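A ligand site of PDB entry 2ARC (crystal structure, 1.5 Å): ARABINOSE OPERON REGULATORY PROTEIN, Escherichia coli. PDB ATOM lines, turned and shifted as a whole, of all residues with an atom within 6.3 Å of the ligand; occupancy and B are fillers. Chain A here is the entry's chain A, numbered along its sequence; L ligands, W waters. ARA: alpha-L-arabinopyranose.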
ATOM      1  N   ASP A   1     -15.124 -25.256   9.052  1.00  0.00           N
ATOM      2  CA  ASP A   1     -13.728 -24.995   8.591  1.00  0.00           C
ATOM      3  C   ASP A   1     -12.771 -25.237   9.760  1.00  0.00           C
ATOM      4  O   ASP A   1     -12.801 -24.506  10.749  1.00  0.00           O
ATOM      5  CB  ASP A   1     -13.587 -23.536   8.108  1.00  0.00           C
ATOM      6  CG  ASP A   1     -12.226 -23.242   7.514  1.00  0.00           C
ATOM      7  OD1 ASP A   1     -11.345 -24.123   7.555  1.00  0.00           O
ATOM      8  OD2 ASP A   1     -12.035 -22.120   7.008  1.00  0.00           O
ATOM      9  N   PRO A   2     -11.921 -26.282   9.671  1.00  0.00           N
ATOM     10  CA  PRO A   2     -11.010 -26.519  10.793  1.00  0.00           C
ATOM     11  C   PRO A   2     -10.060 -25.356  11.015  1.00  0.00           C
ATOM     12  O   PRO A   2      -9.546 -25.193  12.117  1.00  0.00           O
ATOM     13  CB  PRO A   2     -10.291 -27.820  10.384  1.00  0.00           C
ATOM     14  CG  PRO A   2     -10.301 -27.763   8.889  1.00  0.00           C
ATOM     15  CD  PRO A   2     -11.713 -27.283   8.611  1.00  0.00           C
ATOM     16  N   LEU A   3      -9.890 -24.520   9.986  1.00  0.00           N
ATOM     17  CA  LEU A   3      -9.018 -23.355  10.046  1.00  0.00           C
ATOM     18  C   LEU A   3      -9.578 -22.242  10.913  1.00  0.00           C
ATOM     19  O   LEU A   3      -8.900 -21.267  11.219  1.00  0.00           O
ATOM     20  CB  LEU A   3      -8.741 -22.798   8.638  1.00  0.00           C
ATOM     21  CG  LEU A   3      -8.007 -23.705   7.665  1.00  0.00           C
ATOM     22  CD1 LEU A   3      -7.611 -22.932   6.406  1.00  0.00           C
ATOM     23  CD2 LEU A   3      -6.765 -24.272   8.355  1.00  0.00           C
ATOM     24  N   LEU A   4     -10.833 -22.394  11.314  1.00  0.00           N
ATOM     25  CA  LEU A   4     -11.482 -21.392  12.140  1.00  0.00           C
ATOM     26  C   LEU A   4     -11.860 -21.984  13.472  1.00  0.00           C
ATOM     27  O   LEU A   4     -12.180 -23.175  13.557  1.00  0.00           O
ATOM     28  CB  LEU A   4     -12.719 -20.824  11.437  1.00  0.00           C
ATOM     29  CG  LEU A   4     -12.416 -20.075  10.137  1.00  0.00           C
ATOM     30  CD1 LEU A   4     -13.699 -19.670   9.458  1.00  0.00           C
ATOM     31  CD2 LEU A   4     -11.547 -18.844  10.418  1.00  0.00           C
ATOM     32  N   PRO A   5     -11.776 -21.182  14.546  1.00  0.00           N
ATOM     33  CA  PRO A   5     -12.126 -21.635  15.896  1.00  0.00           C
ATOM     34  C   PRO A   5     -13.550 -22.197  15.991  1.00  0.00           C
ATOM     35  O   PRO A   5     -14.410 -21.884  15.152  1.00  0.00           O
ATOM     36  CB  PRO A   5     -11.948 -20.365  16.744  1.00  0.00           C
ATOM     37  CG  PRO A   5     -12.040 -19.230  15.740  1.00  0.00           C
ATOM     38  CD  PRO A   5     -11.306 -19.783  14.559  1.00  0.00           C
ATOM     39  N   PHE A   9     -12.612 -31.002  16.928  1.00  0.00           N
ATOM     40  CA  PHE A   9     -11.565 -31.988  16.725  1.00  0.00           C
ATOM     41  C   PHE A   9     -11.794 -33.109  17.761  1.00  0.00           C
ATOM     42  O   PHE A   9     -11.732 -32.852  18.966  1.00  0.00           O
ATOM     43  CB  PHE A   9     -10.183 -31.358  16.982  1.00  0.00           C
ATOM     44  CG  PHE A   9      -9.757 -30.367  15.943  1.00  0.00           C
ATOM     45  CD1 PHE A   9      -9.129 -30.787  14.764  1.00  0.00           C
ATOM     46  CD2 PHE A   9      -9.904 -28.998  16.170  1.00  0.00           C
ATOM     47  CE1 PHE A   9      -8.668 -29.855  13.826  1.00  0.00           C
ATOM     48  CE2 PHE A   9      -9.443 -28.053  15.225  1.00  0.00           C
ATOM     49  CZ  PHE A   9      -8.820 -28.474  14.060  1.00  0.00           C
ATOM     50  N   THR A  18      -2.446 -24.106   7.004  1.00  0.00           N
ATOM     51  CA  THR A  18      -2.954 -22.822   7.458  1.00  0.00           C
ATOM     52  C   THR A  18      -2.007 -21.770   6.862  1.00  0.00           C
ATOM     53  O   THR A  18      -0.881 -21.557   7.360  1.00  0.00           O
ATOM     54  CB  THR A  18      -2.964 -22.741   8.991  1.00  0.00           C
ATOM     55  OG1 THR A  18      -3.688 -23.862   9.517  1.00  0.00           O
ATOM     56  CG2 THR A  18      -3.641 -21.455   9.445  1.00  0.00           C
ATOM     57  N   ILE A  20      -1.275 -18.516   6.862  1.00  0.00           N
ATOM     58  CA  ILE A  20      -1.474 -17.220   7.505  1.00  0.00           C
ATOM     59  C   ILE A  20      -0.703 -16.108   6.774  1.00  0.00           C
ATOM     60  O   ILE A  20       0.521 -16.192   6.627  1.00  0.00           O
ATOM     61  CB  ILE A  20      -1.054 -17.197   8.991  1.00  0.00           C
ATOM     62  CG1 ILE A  20      -1.840 -18.255   9.784  1.00  0.00           C
ATOM     63  CG2 ILE A  20      -1.305 -15.793   9.572  1.00  0.00           C
ATOM     64  CD1 ILE A  20      -1.361 -18.436  11.226  1.00  0.00           C
ATOM     65  N   PHE A  28      -4.735 -14.553  13.059  1.00  0.00           N
ATOM     66  CA  PHE A  28      -5.104 -14.548  14.467  1.00  0.00           C
ATOM     67  C   PHE A  28      -4.384 -15.722  15.124  1.00  0.00           C
ATOM     68  O   PHE A  28      -3.920 -16.641  14.438  1.00  0.00           O
ATOM     69  CB  PHE A  28      -6.624 -14.666  14.655  1.00  0.00           C
ATOM     70  CG  PHE A  28      -7.226 -15.899  14.060  1.00  0.00           C
ATOM     71  CD1 PHE A  28      -7.246 -17.108  14.772  1.00  0.00           C
ATOM     72  CD2 PHE A  28      -7.765 -15.878  12.776  1.00  0.00           C
ATOM     73  CE1 PHE A  28      -7.780 -18.264  14.214  1.00  0.00           C
ATOM     74  CE2 PHE A  28      -8.303 -17.030  12.208  1.00  0.00           C
ATOM     75  CZ  PHE A  28      -8.313 -18.225  12.934  1.00  0.00           C
ATOM     76  N   ILE A  30      -4.104 -19.106  17.172  1.00  0.00           N
ATOM     77  CA  ILE A  30      -4.761 -20.247  17.778  1.00  0.00           C
ATOM     78  C   ILE A  30      -4.620 -20.237  19.303  1.00  0.00           C
ATOM     79  O   ILE A  30      -3.606 -19.809  19.870  1.00  0.00           O
ATOM     80  CB  ILE A  30      -4.227 -21.608  17.203  1.00  0.00           C
ATOM     81  CG1 ILE A  30      -4.529 -21.744  15.706  1.00  0.00           C
ATOM     82  CG2 ILE A  30      -4.857 -22.764  17.964  1.00  0.00           C
ATOM     83  CD1 ILE A  30      -3.609 -20.947  14.818  1.00  0.00           C
ATOM     84  N   ARG A  32      -5.950 -22.405  22.531  1.00  0.00           N
ATOM     85  CA  ARG A  32      -6.642 -23.509  23.210  1.00  0.00           C
ATOM     86  C   ARG A  32      -5.849 -23.672  24.499  1.00  0.00           C
ATOM     87  O   ARG A  32      -4.949 -24.498  24.599  1.00  0.00           O
ATOM     88  CB  ARG A  32      -6.585 -24.782  22.358  1.00  0.00           C
ATOM     89  CG  ARG A  32      -7.110 -24.571  20.946  1.00  0.00           C
ATOM     90  CD  ARG A  32      -7.070 -25.822  20.075  1.00  0.00           C
ATOM     91  NE  ARG A  32      -7.534 -25.444  18.737  1.00  0.00           N
ATOM     92  CZ  ARG A  32      -6.929 -25.722  17.587  1.00  0.00           C
ATOM     93  NH1 ARG A  32      -5.796 -26.421  17.551  1.00  0.00           N
ATOM     94  NH2 ARG A  32      -7.378 -25.138  16.492  1.00  0.00           N
ATOM     95  N   MET A  36      -6.067 -30.038  23.847  1.00  0.00           N
ATOM     96  CA  MET A  36      -6.981 -30.886  23.090  1.00  0.00           C
ATOM     97  C   MET A  36      -6.906 -32.336  23.547  1.00  0.00           C
ATOM     98  O   MET A  36      -6.033 -32.695  24.339  1.00  0.00           O
ATOM     99  CB  MET A  36      -6.638 -30.818  21.595  1.00  0.00           C
ATOM    100  CG  MET A  36      -6.381 -29.417  21.100  1.00  0.00           C
ATOM    101  SD  MET A  36      -5.863 -29.341  19.378  1.00  0.00           S
ATOM    102  CE  MET A  36      -7.460 -29.362  18.571  1.00  0.00           C
ATOM    103  N   ILE A  40      -1.204 -32.864  17.887  1.00  0.00           N
ATOM    104  CA  ILE A  40      -1.051 -32.082  16.660  1.00  0.00           C
ATOM    105  C   ILE A  40       0.442 -31.991  16.312  1.00  0.00           C
ATOM    106  O   ILE A  40       1.277 -31.681  17.170  1.00  0.00           O
ATOM    107  CB  ILE A  40      -1.649 -30.655  16.702  1.00  0.00           C
ATOM    108  CG1 ILE A  40      -3.188 -30.753  16.700  1.00  0.00           C
ATOM    109  CG2 ILE A  40      -1.176 -29.850  15.470  1.00  0.00           C
ATOM    110  CD1 ILE A  40      -3.927 -29.488  16.314  1.00  0.00           C
ATOM    111  N   ASN A  42       3.053 -30.140  13.718  1.00  0.00           N
ATOM    112  CA  ASN A  42       3.012 -28.887  12.955  1.00  0.00           C
ATOM    113  C   ASN A  42       4.356 -28.660  12.261  1.00  0.00           C
ATOM    114  O   ASN A  42       5.393 -28.761  12.881  1.00  0.00           O
ATOM    115  CB  ASN A  42       2.683 -27.757  13.964  1.00  0.00           C
ATOM    116  CG  ASN A  42       2.760 -26.348  13.374  1.00  0.00           C
ATOM    117  OD1 ASN A  42       3.751 -25.963  12.745  1.00  0.00           O
ATOM    118  ND2 ASN A  42       1.757 -25.524  13.691  1.00  0.00           N
ATOM    119  N   HIS A  74      -2.211 -24.711  23.429  1.00  0.00           N
ATOM    120  CA  HIS A  74      -1.975 -24.316  22.033  1.00  0.00           C
ATOM    121  C   HIS A  74      -2.132 -22.801  22.034  1.00  0.00           C
ATOM    122  O   HIS A  74      -3.200 -22.293  22.360  1.00  0.00           O
ATOM    123  CB  HIS A  74      -3.010 -24.871  21.036  1.00  0.00           C
ATOM    124  CG  HIS A  74      -2.867 -26.321  20.745  1.00  0.00           C
ATOM    125  ND1 HIS A  74      -2.639 -26.797  19.466  1.00  0.00           N
ATOM    126  CD2 HIS A  74      -2.966 -27.416  21.544  1.00  0.00           C
ATOM    127  CE1 HIS A  74      -2.606 -28.117  19.497  1.00  0.00           C
ATOM    128  NE2 HIS A  74      -2.805 -28.518  20.738  1.00  0.00           N
ATOM    129  N   TYR A  76      -0.404 -20.027  19.495  1.00  0.00           N
ATOM    130  CA  TYR A  76       0.571 -19.700  18.462  1.00  0.00           C
ATOM    131  C   TYR A  76      -0.056 -18.989  17.271  1.00  0.00           C
ATOM    132  O   TYR A  76      -1.257 -19.125  17.004  1.00  0.00           O
ATOM    133  CB  TYR A  76       1.312 -20.966  18.013  1.00  0.00           C
ATOM    134  CG  TYR A  76       0.428 -22.184  17.788  1.00  0.00           C
ATOM    135  CD1 TYR A  76      -0.378 -22.291  16.642  1.00  0.00           C
ATOM    136  CD2 TYR A  76       0.408 -23.251  18.715  1.00  0.00           C
ATOM    137  CE1 TYR A  76      -1.153 -23.439  16.423  1.00  0.00           C
ATOM    138  CE2 TYR A  76      -0.361 -24.380  18.501  1.00  0.00           C
ATOM    139  CZ  TYR A  76      -1.140 -24.476  17.360  1.00  0.00           C
ATOM    140  OH  TYR A  76      -1.891 -25.609  17.137  1.00  0.00           O
ATOM    141  N   TRP A  85       2.922 -16.906   7.951  1.00  0.00           N
ATOM    142  CA  TRP A  85       3.292 -18.107   8.670  1.00  0.00           C
ATOM    143  C   TRP A  85       2.420 -19.216   8.117  1.00  0.00           C
ATOM    144  O   TRP A  85       1.269 -19.396   8.533  1.00  0.00           O
ATOM    145  CB  TRP A  85       3.131 -18.015  10.188  1.00  0.00           C
ATOM    146  CG  TRP A  85       3.568 -19.325  10.861  1.00  0.00           C
ATOM    147  CD1 TRP A  85       4.632 -20.125  10.494  1.00  0.00           C
ATOM    148  CD2 TRP A  85       2.928 -20.000  11.969  1.00  0.00           C
ATOM    149  NE1 TRP A  85       4.699 -21.227  11.315  1.00  0.00           N
ATOM    150  CE2 TRP A  85       3.669 -21.181  12.227  1.00  0.00           C
ATOM    151  CE3 TRP A  85       1.806 -19.711  12.771  1.00  0.00           C
ATOM    152  CZ2 TRP A  85       3.324 -22.087  13.254  1.00  0.00           C
ATOM    153  CZ3 TRP A  85       1.477 -20.613  13.805  1.00  0.00           C
ATOM    154  CH2 TRP A  85       2.240 -21.783  14.035  1.00  0.00           C
ATOM    155  N   HIS A  87       1.817 -23.046   7.776  1.00  0.00           N
ATOM    156  CA  HIS A  87       2.201 -24.265   8.460  1.00  0.00           C
ATOM    157  C   HIS A  87       1.246 -25.375   8.111  1.00  0.00           C
ATOM    158  O   HIS A  87       0.051 -25.118   7.912  1.00  0.00           O
ATOM    159  CB  HIS A  87       2.242 -24.062   9.996  1.00  0.00           C
ATOM    160  CG  HIS A  87       0.933 -23.618  10.600  1.00  0.00           C
ATOM    161  ND1 HIS A  87       0.591 -22.286  10.721  1.00  0.00           N
ATOM    162  CD2 HIS A  87      -0.057 -24.322  11.209  1.00  0.00           C
ATOM    163  CE1 HIS A  87      -0.547 -22.185  11.388  1.00  0.00           C
ATOM    164  NE2 HIS A  87      -0.961 -23.410  11.692  1.00  0.00           N
ATOM    165  N   TRP A  89      -0.354 -29.059   9.245  1.00  0.00           N
ATOM    166  CA  TRP A  89      -0.600 -29.655  10.546  1.00  0.00           C
ATOM    167  C   TRP A  89      -1.490 -30.887  10.432  1.00  0.00           C
ATOM    168  O   TRP A  89      -2.225 -31.048   9.455  1.00  0.00           O
ATOM    169  CB  TRP A  89      -1.287 -28.608  11.462  1.00  0.00           C
ATOM    170  CG  TRP A  89      -2.511 -27.973  10.824  1.00  0.00           C
ATOM    171  CD1 TRP A  89      -2.537 -26.843  10.054  1.00  0.00           C
ATOM    172  CD2 TRP A  89      -3.850 -28.496  10.819  1.00  0.00           C
ATOM    173  NE1 TRP A  89      -3.800 -26.653   9.559  1.00  0.00           N
ATOM    174  CE2 TRP A  89      -4.632 -27.645  10.018  1.00  0.00           C
ATOM    175  CE3 TRP A  89      -4.463 -29.617  11.415  1.00  0.00           C
ATOM    176  CZ2 TRP A  89      -5.993 -27.865   9.784  1.00  0.00           C
ATOM    177  CZ3 TRP A  89      -5.812 -29.842  11.185  1.00  0.00           C
ATOM    178  CH2 TRP A  89      -6.570 -28.964  10.373  1.00  0.00           C
ATOM    179  N   TYR A  91      -3.886 -33.345  13.132  1.00  0.00           N
ATOM    180  CA  TYR A  91      -4.497 -33.651  14.416  1.00  0.00           C
ATOM    181  C   TYR A  91      -4.746 -35.165  14.395  1.00  0.00           C
ATOM    182  O   TYR A  91      -5.349 -35.672  13.449  1.00  0.00           O
ATOM    183  CB  TYR A  91      -5.836 -32.888  14.559  1.00  0.00           C
ATOM    184  CG  TYR A  91      -6.643 -33.315  15.772  1.00  0.00           C
ATOM    185  CD1 TYR A  91      -6.388 -32.769  17.033  1.00  0.00           C
ATOM    186  CD2 TYR A  91      -7.614 -34.316  15.666  1.00  0.00           C
ATOM    187  CE1 TYR A  91      -7.075 -33.220  18.177  1.00  0.00           C
ATOM    188  CE2 TYR A  91      -8.308 -34.773  16.799  1.00  0.00           C
ATOM    189  CZ  TYR A  91      -8.032 -34.222  18.054  1.00  0.00           C
ATOM    190  OH  TYR A  91      -8.679 -34.679  19.168  1.00  0.00           O
HETATM  191  C1  ARA L   1      -6.348 -25.032  12.849  1.00  0.00           C
HETATM  192  C2  ARA L   1      -4.981 -24.339  13.090  1.00  0.00           C
HETATM  193  C3  ARA L   1      -3.849 -25.358  13.126  1.00  0.00           C
HETATM  194  C4  ARA L   1      -4.154 -26.482  14.100  1.00  0.00           C
HETATM  195  C5  ARA L   1      -5.523 -27.087  13.768  1.00  0.00           C
HETATM  196  O1  ARA L   1      -7.384 -24.116  13.009  1.00  0.00           O
HETATM  197  O2  ARA L   1      -4.719 -23.382  12.058  1.00  0.00           O
HETATM  198  O3  ARA L   1      -2.626 -24.724  13.495  1.00  0.00           O
HETATM  199  O4  ARA L   1      -4.132 -26.009  15.450  1.00  0.00           O
HETATM  200  O5  ARA L   1      -6.551 -26.079  13.811  1.00  0.00           O
HETATM  201  O   HOH W   1      -8.178 -21.838  14.484  1.00  0.00           O
HETATM  202  O   HOH W   2      -6.252 -21.135  12.161  1.00  0.00           O
HETATM  203  O   HOH W   3      -0.717 -26.347  14.611  1.00  0.00           O
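The backbone carbonyl oxygen of Pro 2 sits at hydrogen-bond distance from an oxygen (O1) of the ligand. The guanidinium group (NH1) of Arg 32 sits at hydrogen-bond distance from an oxygen (O4) of the ligand, at 2.7 Å. A ring nitrogen (NE2) of His 87 sits at hydrogen-bond distance from an oxygen (O3) of the ligand. The side-chain hydroxyl (OG1) of Thr 18 sits at hydrogen-bond distance from an oxygen (O2) of the ligand (2.8 Å). OH of Tyr 76 is in hydrogen-bond range of O4 of the ligand (2.8 Å).
Leu 3 touches the ligand. CZ of Phe 9 touches O5 of the ligand, at 3.3 Å. Ile 30 touches the ligand (CG1 to C2, 3.7 Å). CD1 of Ile 40 touches O4 of the ligand, at 3.6 Å. Trp 89 touches the ligand (CE3 to C5, 3.6 Å). Hydrophobic or aromatic side chains that line the ligand: Phe 9, Ile 30, Ile 40, Tyr 76, His 87 and Trp 89. Ten residues have an atom within 4 Å of the ligand: Pro 2, Leu 3, Phe 9, Thr 18, Ile 30, Arg 32, Ile 40, Tyr 76, His 87 and Trp 89.
The backbone NH of Arg 32 sits at hydrogen-bond distance from the backbone carbonyl oxygen of His 74. SD of Met 36 lies within hydrogen-bond range of NH1 of Arg 32, 3.4 Å away. The backbone carbonyl oxygen of His 87 sits at hydrogen-bond distance from the backbone NH of Thr 18. The side-chain hydroxyl (OG1) of Thr 18 lies within hydrogen-bond range of the indole nitrogen (NE1) of Trp 89, 2.8 Å away. O of Tyr 76 sits at hydrogen-bond distance from N of Ile 30 (2.9 Å). The side-chain hydroxyl of Tyr 76 sits at hydrogen-bond distance from a ring nitrogen (ND1) of His 74 (2.7 Å). The backbone NH of Leu 3 sits at hydrogen-bond distance from the side-chain carboxylate of Asp 1 (2.9 Å).
Water W2 lies within hydrogen-bond range of O2 of the ligand (2.7 Å) and O of Leu 3 (2.8 Å). Water W3 lies within hydrogen-bond range of an oxygen (O3) of the ligand, the side-chain amide nitrogen of Asn 42 and the side-chain hydroxyl of Tyr 76. Water W1 bridges an oxygen (O1) of the ligand and the backbone carbonyl oxygen of Leu 3.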
